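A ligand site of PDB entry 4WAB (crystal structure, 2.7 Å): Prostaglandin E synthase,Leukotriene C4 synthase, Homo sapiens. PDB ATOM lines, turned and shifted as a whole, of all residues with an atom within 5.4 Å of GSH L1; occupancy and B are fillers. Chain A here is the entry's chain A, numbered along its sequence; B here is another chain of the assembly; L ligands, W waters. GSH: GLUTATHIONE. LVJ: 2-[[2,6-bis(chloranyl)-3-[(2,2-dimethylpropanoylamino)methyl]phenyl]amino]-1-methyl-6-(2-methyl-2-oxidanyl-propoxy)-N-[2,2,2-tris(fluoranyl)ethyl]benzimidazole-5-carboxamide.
N4 of LVJ L2 lies close to SG2 of GSH L1.
NH2 of Arg 68 is in hydrogen-bond range of OD1 of Asn 44 of chain B, 2.5 Å away.
The guanidinium group (NE) of Arg 71 lies within salt-bridge range of the side-chain carboxylate (OE2) of Glu 75, at 3.0 Å.
The side-chain amide nitrogen (ND2) of Asn 44 of chain B lies close to the guanidinium group (NH2) of Arg 124, 2.9 Å away.
The guanidinium group (NE) of Arg 68 lies within hydrogen-bond range of the side-chain hydroxyl (OH) of Tyr 115 (2.6 Å).
NH2 of Arg 68 lies within hydrogen-bond range of O of Ala 43 of chain B (3.4 Å).
OH of Tyr 115 sits at hydrogen-bond distance from ND2 of Asn 44 of chain B, 3.2 Å away.
CB of Arg 68 touches O32 of GSH L1, 3.6 Å away.
Tyr 128 touches GSH L1.
O of Ala 29 of chain B touches CG1 of GSH L1 (3.7 Å).
Thr 32 of chain B touches GSH L1.
Leu 67 of chain B touches GSH L1.
13 residues have an atom within 4 Å of GSH L1: Arg 68, Arg 71, Asn 72, Glu 75, His 111, Tyr 115, Arg 124, Ser 125, Tyr 128, Ala 29 of chain B, Thr 32 of chain B, Arg 36 of chain B and Leu 67 of chain B.
The nearest printed residue that does not touch GSH L1 is His 70 of chain B (4.3 Å).
OE1 of Glu 75 is in salt-bridge range of N1 of GSH L1, 3.1 Å away.
O2 of GSH L1 lies close to NH1 of Arg 124 (3.3 Å).
The guanidinium group (NH2) of Arg 71 lies within salt-bridge range of an oxygen (O31) of GSH L1 (2.6 Å).
NH2 of Arg 36 of chain B is in salt-bridge range of O12 of GSH L1, at 3.2 Å.
O31 of GSH L1 sits at hydrogen-bond distance from ND2 of Asn 72 (3.1 Å).
The side-chain hydroxyl (OH) of Tyr 115 is in hydrogen-bond range of an oxygen (O32) of GSH L1 (2.6 Å).
OG of Ser 125 sits at hydrogen-bond distance from N1 of LVJ L2 (2.8 Å).
A ring nitrogen (NE2) of His 111 is in hydrogen-bond range of an oxygen (O2) of GSH L1, 2.9 Å away.
A sulfur (SG2) of GSH L1 sits close to the side-chain hydroxyl (OG) of Ser 125 (3.0 Å).
Water W1 lies within hydrogen-bond range of a ring nitrogen (ND1) of His 70 of chain B (2.8 Å), the side-chain hydroxyl (OG1) of Thr 32 of chain B (2.9 Å) and a nitrogen (N1) of GSH L1 (3.0 Å).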
ATOM      1  N   ARG A  68       8.743 -34.765  17.959  1.00  0.00           N
ATOM      2  CA  ARG A  68       8.212 -34.117  19.170  1.00  0.00           C
ATOM      3  C   ARG A  68       6.863 -34.708  19.547  1.00  0.00           C
ATOM      4  O   ARG A  68       6.566 -34.883  20.728  1.00  0.00           O
ATOM      5  CB  ARG A  68       8.074 -32.600  18.983  1.00  0.00           C
ATOM      6  CG  ARG A  68       9.390 -31.913  18.910  1.00  0.00           C
ATOM      7  CD  ARG A  68       9.310 -30.448  19.258  1.00  0.00           C
ATOM      8  NE  ARG A  68       8.464 -29.684  18.354  1.00  0.00           N
ATOM      9  CZ  ARG A  68       8.830 -29.253  17.156  1.00  0.00           C
ATOM     10  NH1 ARG A  68      10.059 -29.510  16.688  1.00  0.00           N
ATOM     11  NH2 ARG A  68       7.979 -28.557  16.407  1.00  0.00           N
ATOM     12  N   ALA A  69       6.072 -35.005  18.526  1.00  0.00           N
ATOM     13  CA  ALA A  69       4.757 -35.630  18.704  1.00  0.00           C
ATOM     14  C   ALA A  69       4.897 -37.039  19.255  1.00  0.00           C
ATOM     15  O   ALA A  69       4.200 -37.439  20.193  1.00  0.00           O
ATOM     16  CB  ALA A  69       4.022 -35.661  17.391  1.00  0.00           C
ATOM     17  N   ARG A  71       7.549 -38.208  20.858  1.00  0.00           N
ATOM     18  CA  ARG A  71       8.115 -38.157  22.205  1.00  0.00           C
ATOM     19  C   ARG A  71       7.050 -37.847  23.258  1.00  0.00           C
ATOM     20  O   ARG A  71       6.963 -38.524  24.294  1.00  0.00           O
ATOM     21  CB  ARG A  71       9.222 -37.124  22.293  1.00  0.00           C
ATOM     22  CG  ARG A  71      10.051 -37.271  23.584  1.00  0.00           C
ATOM     23  CD  ARG A  71      10.704 -35.984  23.954  1.00  0.00           C
ATOM     24  NE  ARG A  71       9.725 -34.903  23.989  1.00  0.00           N
ATOM     25  CZ  ARG A  71       9.764 -33.829  23.210  1.00  0.00           C
ATOM     26  NH1 ARG A  71      10.751 -33.690  22.329  1.00  0.00           N
ATOM     27  NH2 ARG A  71       8.833 -32.906  23.316  1.00  0.00           N
ATOM     28  N   ASN A  72       6.246 -36.833  22.983  1.00  0.00           N
ATOM     29  CA  ASN A  72       5.110 -36.518  23.842  1.00  0.00           C
ATOM     30  C   ASN A  72       4.150 -37.715  24.050  1.00  0.00           C
ATOM     31  O   ASN A  72       3.564 -37.848  25.132  1.00  0.00           O
ATOM     32  CB  ASN A  72       4.344 -35.312  23.266  1.00  0.00           C
ATOM     33  CG  ASN A  72       3.392 -34.702  24.269  1.00  0.00           C
ATOM     34  OD1 ASN A  72       2.278 -35.197  24.495  1.00  0.00           O
ATOM     35  ND2 ASN A  72       3.821 -33.613  24.886  1.00  0.00           N
ATOM     36  N   GLU A  75       5.596 -39.799  26.603  1.00  0.00           N
ATOM     37  CA  GLU A  75       5.567 -39.237  27.939  1.00  0.00           C
ATOM     38  C   GLU A  75       4.184 -39.302  28.554  1.00  0.00           C
ATOM     39  O   GLU A  75       4.004 -39.061  29.744  1.00  0.00           O
ATOM     40  CB  GLU A  75       6.064 -37.797  27.939  1.00  0.00           C
ATOM     41  CG  GLU A  75       7.410 -37.541  27.276  1.00  0.00           C
ATOM     42  CD  GLU A  75       7.678 -36.050  27.082  1.00  0.00           C
ATOM     43  OE1 GLU A  75       6.728 -35.250  27.257  1.00  0.00           O
ATOM     44  OE2 GLU A  75       8.825 -35.667  26.777  1.00  0.00           O
ATOM     45  N   HIS A 111      -4.638 -34.646  20.158  1.00  0.00           N
ATOM     46  CA  HIS A 111      -3.328 -34.031  20.393  1.00  0.00           C
ATOM     47  C   HIS A 111      -2.458 -34.112  19.164  1.00  0.00           C
ATOM     48  O   HIS A 111      -1.875 -33.112  18.741  1.00  0.00           O
ATOM     49  CB  HIS A 111      -2.591 -34.713  21.554  1.00  0.00           C
ATOM     50  CG  HIS A 111      -1.318 -34.010  21.958  1.00  0.00           C
ATOM     51  ND1 HIS A 111      -0.085 -34.340  21.419  1.00  0.00           N
ATOM     52  CD2 HIS A 111      -1.081 -33.019  22.842  1.00  0.00           C
ATOM     53  CE1 HIS A 111       0.846 -33.568  21.959  1.00  0.00           C
ATOM     54  NE2 HIS A 111       0.266 -32.752  22.816  1.00  0.00           N
ATOM     55  N   TYR A 115      -0.821 -31.372  16.550  1.00  0.00           N
ATOM     56  CA  TYR A 115       0.619 -31.190  16.382  1.00  0.00           C
ATOM     57  C   TYR A 115       0.995 -31.306  14.905  1.00  0.00           C
ATOM     58  O   TYR A 115       1.602 -30.381  14.319  1.00  0.00           O
ATOM     59  CB  TYR A 115       1.411 -32.219  17.214  1.00  0.00           C
ATOM     60  CG  TYR A 115       2.703 -31.670  17.822  1.00  0.00           C
ATOM     61  CD1 TYR A 115       3.067 -31.984  19.117  1.00  0.00           C
ATOM     62  CD2 TYR A 115       3.509 -30.801  17.109  1.00  0.00           C
ATOM     63  CE1 TYR A 115       4.237 -31.497  19.678  1.00  0.00           C
ATOM     64  CE2 TYR A 115       4.680 -30.285  17.675  1.00  0.00           C
ATOM     65  CZ  TYR A 115       5.044 -30.643  18.966  1.00  0.00           C
ATOM     66  OH  TYR A 115       6.183 -30.176  19.571  1.00  0.00           O
ATOM     67  N   ARG A 124      -3.365 -27.494  20.871  1.00  0.00           N
ATOM     68  CA  ARG A 124      -2.681 -28.720  21.288  1.00  0.00           C
ATOM     69  C   ARG A 124      -2.501 -28.730  22.797  1.00  0.00           C
ATOM     70  O   ARG A 124      -2.732 -29.732  23.462  1.00  0.00           O
ATOM     71  CB  ARG A 124      -1.323 -28.886  20.625  1.00  0.00           C
ATOM     72  CG  ARG A 124      -0.338 -29.598  21.534  1.00  0.00           C
ATOM     73  CD  ARG A 124       1.003 -29.903  20.917  1.00  0.00           C
ATOM     74  NE  ARG A 124       1.559 -28.686  20.365  1.00  0.00           N
ATOM     75  CZ  ARG A 124       2.187 -27.726  21.031  1.00  0.00           C
ATOM     76  NH1 ARG A 124       2.351 -27.766  22.356  1.00  0.00           N
ATOM     77  NH2 ARG A 124       2.630 -26.693  20.356  1.00  0.00           N
ATOM     78  N   SER A 125      -2.090 -27.581  23.331  1.00  0.00           N
ATOM     79  CA  SER A 125      -1.701 -27.465  24.731  1.00  0.00           C
ATOM     80  C   SER A 125      -2.882 -27.821  25.658  1.00  0.00           C
ATOM     81  O   SER A 125      -2.685 -28.472  26.691  1.00  0.00           O
ATOM     82  CB  SER A 125      -1.171 -26.059  25.011  1.00  0.00           C
ATOM     83  OG  SER A 125      -0.471 -26.014  26.236  1.00  0.00           O
ATOM     84  N   TYR A 128      -3.580 -31.653  25.441  1.00  0.00           N
ATOM     85  CA  TYR A 128      -2.631 -32.367  26.301  1.00  0.00           C
ATOM     86  C   TYR A 128      -3.145 -32.399  27.755  1.00  0.00           C
ATOM     87  O   TYR A 128      -3.108 -33.440  28.426  1.00  0.00           O
ATOM     88  CB  TYR A 128      -1.238 -31.735  26.230  1.00  0.00           C
ATOM     89  CG  TYR A 128      -0.351 -32.151  27.373  1.00  0.00           C
ATOM     90  CD1 TYR A 128       0.446 -33.281  27.289  1.00  0.00           C
ATOM     91  CD2 TYR A 128      -0.341 -31.435  28.577  1.00  0.00           C
ATOM     92  CE1 TYR A 128       1.227 -33.682  28.350  1.00  0.00           C
ATOM     93  CE2 TYR A 128       0.435 -31.838  29.630  1.00  0.00           C
ATOM     94  CZ  TYR A 128       1.218 -32.967  29.507  1.00  0.00           C
ATOM     95  OH  TYR A 128       2.002 -33.371  30.544  1.00  0.00           O
ATOM     96  N   ALA B  29       7.364 -32.732  33.778  1.00  0.00           N
ATOM     97  CA  ALA B  29       6.628 -32.183  32.652  1.00  0.00           C
ATOM     98  C   ALA B  29       6.116 -30.767  32.941  1.00  0.00           C
ATOM     99  O   ALA B  29       6.308 -29.866  32.131  1.00  0.00           O
ATOM    100  CB  ALA B  29       5.475 -33.118  32.281  1.00  0.00           C
ATOM    101  N   THR B  32       8.778 -28.312  33.117  1.00  0.00           N
ATOM    102  CA  THR B  32       9.260 -28.057  31.768  1.00  0.00           C
ATOM    103  C   THR B  32       8.471 -26.974  31.030  1.00  0.00           C
ATOM    104  O   THR B  32       9.073 -26.082  30.406  1.00  0.00           O
ATOM    105  CB  THR B  32       9.292 -29.356  30.928  1.00  0.00           C
ATOM    106  OG1 THR B  32      10.323 -30.203  31.438  1.00  0.00           O
ATOM    107  CG2 THR B  32       9.585 -29.070  29.425  1.00  0.00           C
ATOM    108  N   GLY B  33       7.140 -27.032  31.101  1.00  0.00           N
ATOM    109  CA  GLY B  33       6.299 -26.034  30.477  1.00  0.00           C
ATOM    110  C   GLY B  33       6.480 -24.656  31.112  1.00  0.00           C
ATOM    111  O   GLY B  33       6.524 -23.637  30.410  1.00  0.00           O
ATOM    112  N   ARG B  36       9.489 -23.102  29.867  1.00  0.00           N
ATOM    113  CA  ARG B  36       9.250 -22.593  28.522  1.00  0.00           C
ATOM    114  C   ARG B  36       8.557 -21.229  28.551  1.00  0.00           C
ATOM    115  O   ARG B  36       8.923 -20.340  27.772  1.00  0.00           O
ATOM    116  CB  ARG B  36       8.406 -23.581  27.705  1.00  0.00           C
ATOM    117  CG  ARG B  36       9.184 -24.778  27.188  1.00  0.00           C
ATOM    118  CD  ARG B  36       8.396 -25.494  26.137  1.00  0.00           C
ATOM    119  NE  ARG B  36       9.050 -26.732  25.699  1.00  0.00           N
ATOM    120  CZ  ARG B  36       9.929 -26.806  24.697  1.00  0.00           C
ATOM    121  NH1 ARG B  36      10.284 -25.713  24.014  1.00  0.00           N
ATOM    122  NH2 ARG B  36      10.455 -27.987  24.380  1.00  0.00           N
ATOM    123  N   ALA B  43       9.058 -24.742  21.342  1.00  0.00           N
ATOM    124  CA  ALA B  43       9.490 -25.642  20.280  1.00  0.00           C
ATOM    125  C   ALA B  43       8.792 -25.347  18.958  1.00  0.00           C
ATOM    126  O   ALA B  43       9.278 -25.745  17.902  1.00  0.00           O
ATOM    127  CB  ALA B  43       9.252 -27.092  20.670  1.00  0.00           C
ATOM    128  N   ASN B  44       7.676 -24.644  19.023  1.00  0.00           N
ATOM    129  CA  ASN B  44       6.818 -24.486  17.851  1.00  0.00           C
ATOM    130  C   ASN B  44       6.533 -23.040  17.504  1.00  0.00           C
ATOM    131  O   ASN B  44       6.285 -22.240  18.397  1.00  0.00           O
ATOM    132  CB  ASN B  44       5.496 -25.216  18.052  1.00  0.00           C
ATOM    133  CG  ASN B  44       5.673 -26.682  18.395  1.00  0.00           C
ATOM    134  OD1 ASN B  44       6.064 -27.489  17.550  1.00  0.00           O
ATOM    135  ND2 ASN B  44       5.392 -27.033  19.645  1.00  0.00           N
ATOM    136  N   LEU B  67      14.078 -31.493  29.530  1.00  0.00           N
ATOM    137  CA  LEU B  67      13.902 -32.612  28.600  1.00  0.00           C
ATOM    138  C   LEU B  67      14.893 -33.764  28.805  1.00  0.00           C
ATOM    139  O   LEU B  67      14.517 -34.931  28.627  1.00  0.00           O
ATOM    140  CB  LEU B  67      14.018 -32.116  27.160  1.00  0.00           C
ATOM    141  CG  LEU B  67      12.914 -31.181  26.686  1.00  0.00           C
ATOM    142  CD1 LEU B  67      12.860 -31.192  25.180  1.00  0.00           C
ATOM    143  CD2 LEU B  67      11.600 -31.622  27.261  1.00  0.00           C
ATOM    144  N   HIS B  70      13.670 -35.568  31.898  1.00  0.00           N
ATOM    145  CA  HIS B  70      12.482 -36.315  31.524  1.00  0.00           C
ATOM    146  C   HIS B  70      12.826 -37.549  30.691  1.00  0.00           C
ATOM    147  O   HIS B  70      12.268 -38.618  30.914  1.00  0.00           O
ATOM    148  CB  HIS B  70      11.507 -35.413  30.761  1.00  0.00           C
ATOM    149  CG  HIS B  70      10.088 -35.853  30.847  1.00  0.00           C
ATOM    150  ND1 HIS B  70       9.048 -35.077  30.413  1.00  0.00           N
ATOM    151  CD2 HIS B  70       9.537 -37.001  31.314  1.00  0.00           C
ATOM    152  CE1 HIS B  70       7.907 -35.709  30.609  1.00  0.00           C
ATOM    153  NE2 HIS B  70       8.177 -36.890  31.149  1.00  0.00           N
HETATM  154  N1  GSH L   1       8.208 -32.566  27.063  1.00  0.00           N
HETATM  155  CA1 GSH L   1       7.142 -31.557  27.055  1.00  0.00           C
HETATM  156  C1  GSH L   1       7.651 -30.265  26.387  1.00  0.00           C
HETATM  157  O11 GSH L   1       6.719 -29.362  26.206  1.00  0.00           O
HETATM  158  O12 GSH L   1       8.811 -30.113  26.058  1.00  0.00           O
HETATM  159  CB1 GSH L   1       6.630 -31.292  28.523  1.00  0.00           C
HETATM  160  CG1 GSH L   1       5.328 -30.464  28.614  1.00  0.00           C
HETATM  161  CD1 GSH L   1       4.212 -30.975  27.735  1.00  0.00           C
HETATM  162  OE1 GSH L   1       3.963 -32.171  27.618  1.00  0.00           O
HETATM  163  N2  GSH L   1       3.514 -30.028  27.086  1.00  0.00           N
HETATM  164  CA2 GSH L   1       2.403 -30.338  26.203  1.00  0.00           C
HETATM  165  C2  GSH L   1       2.869 -30.541  24.761  1.00  0.00           C
HETATM  166  O2  GSH L   1       2.058 -30.662  23.847  1.00  0.00           O
HETATM  167  CB2 GSH L   1       1.360 -29.233  26.200  1.00  0.00           C
HETATM  168  SG2 GSH L   1       2.007 -27.601  25.741  1.00  0.00           S
HETATM  169  N3  GSH L   1       4.184 -30.549  24.560  1.00  0.00           N
HETATM  170  CA3 GSH L   1       4.713 -30.575  23.213  1.00  0.00           C
HETATM  171  C3  GSH L   1       5.953 -31.417  23.067  1.00  0.00           C
HETATM  172  O31 GSH L   1       6.351 -32.203  23.917  1.00  0.00           O
HETATM  173  O32 GSH L   1       6.539 -31.198  21.923  1.00  0.00           O
HETATM  174  O3  LVJ L   2       3.062 -25.202  30.902  1.00  0.00           O
HETATM  175  C22 LVJ L   2       2.600 -25.970  30.070  1.00  0.00           C
HETATM  176  C23 LVJ L   2       1.691 -27.140  30.454  1.00  0.00           C
HETATM  177  C26 LVJ L   2       1.031 -26.863  31.807  1.00  0.00           C
HETATM  178  C25 LVJ L   2       0.587 -27.303  29.412  1.00  0.00           C
HETATM  179  C24 LVJ L   2       2.509 -28.425  30.549  1.00  0.00           C
HETATM  180  N4  LVJ L   2       2.853 -25.821  28.768  1.00  0.00           N
HETATM  181  C21 LVJ L   2       3.649 -24.724  28.240  1.00  0.00           C
HETATM  182  C19 LVJ L   2       3.018 -24.041  27.053  1.00  0.00           C
HETATM  183  C18 LVJ L   2       3.510 -24.279  25.766  1.00  0.00           C
HETATM  184  C17 LVJ L   2       2.868 -23.745  24.659  1.00  0.00           C
HETATM  185  C16 LVJ L   2       1.741 -22.974  24.823  1.00  0.00           C
HETATM  186 CL   LVJ L   2       0.928 -22.364  23.426  1.00  0.00          CL
HETATM  187  C20 LVJ L   2       1.901 -23.235  27.193  1.00  0.00           C
HETATM  188 CL1  LVJ L   2       1.352 -22.853  28.789  1.00  0.00          CL
HETATM  189  C15 LVJ L   2       1.233 -22.689  26.099  1.00  0.00           C
HETATM  190  N3  LVJ L   2       0.067 -21.880  26.255  1.00  0.00           N
HETATM  191  C1  LVJ L   2      -1.094 -22.315  26.800  1.00  0.00           C
HETATM  192  N1  LVJ L   2      -1.323 -23.518  27.267  1.00  0.00           N
HETATM  193  C2  LVJ L   2      -2.634 -23.487  27.719  1.00  0.00           C
HETATM  194  C11 LVJ L   2      -3.193 -22.223  27.491  1.00  0.00           C
HETATM  195  N   LVJ L   2      -2.171 -21.481  26.900  1.00  0.00           N
HETATM  196  C   LVJ L   2      -2.233 -20.089  26.482  1.00  0.00           C
HETATM  197  C10 LVJ L   2      -4.494 -21.916  27.840  1.00  0.00           C
HETATM  198  C5  LVJ L   2      -5.250 -22.908  28.430  1.00  0.00           C
HETATM  199  O   LVJ L   2      -6.559 -22.731  28.784  1.00  0.00           O
HETATM  200  C6  LVJ L   2      -7.167 -21.451  28.500  1.00  0.00           C
HETATM  201  C7  LVJ L   2      -8.660 -21.576  28.653  1.00  0.00           C
HETATM  202  O1  LVJ L   2      -8.938 -21.941  30.021  1.00  0.00           O
HETATM  203  C9  LVJ L   2      -9.209 -22.670  27.744  1.00  0.00           C
HETATM  204  C8  LVJ L   2      -9.345 -20.240  28.368  1.00  0.00           C
HETATM  205  C4  LVJ L   2      -4.717 -24.190  28.711  1.00  0.00           C
HETATM  206  C3  LVJ L   2      -3.404 -24.471  28.327  1.00  0.00           C
HETATM  207  C12 LVJ L   2      -5.406 -25.302  29.436  1.00  0.00           C
HETATM  208  O2  LVJ L   2      -4.906 -26.424  29.461  1.00  0.00           O
HETATM  209  N2  LVJ L   2      -6.528 -25.009  30.093  1.00  0.00           N
HETATM  210  C13 LVJ L   2      -7.155 -25.923  31.039  1.00  0.00           C
HETATM  211  C14 LVJ L   2      -8.197 -26.827  30.284  1.00  0.00           C
HETATM  212  F   LVJ L   2      -8.913 -27.558  31.106  1.00  0.00           F
HETATM  213  F1  LVJ L   2      -7.609 -27.669  29.438  1.00  0.00           F
HETATM  214  F2  LVJ L   2      -9.054 -26.101  29.555  1.00  0.00           F
HETATM  215  O   HOH W   1       9.743 -32.456  29.664  1.00  0.00           O
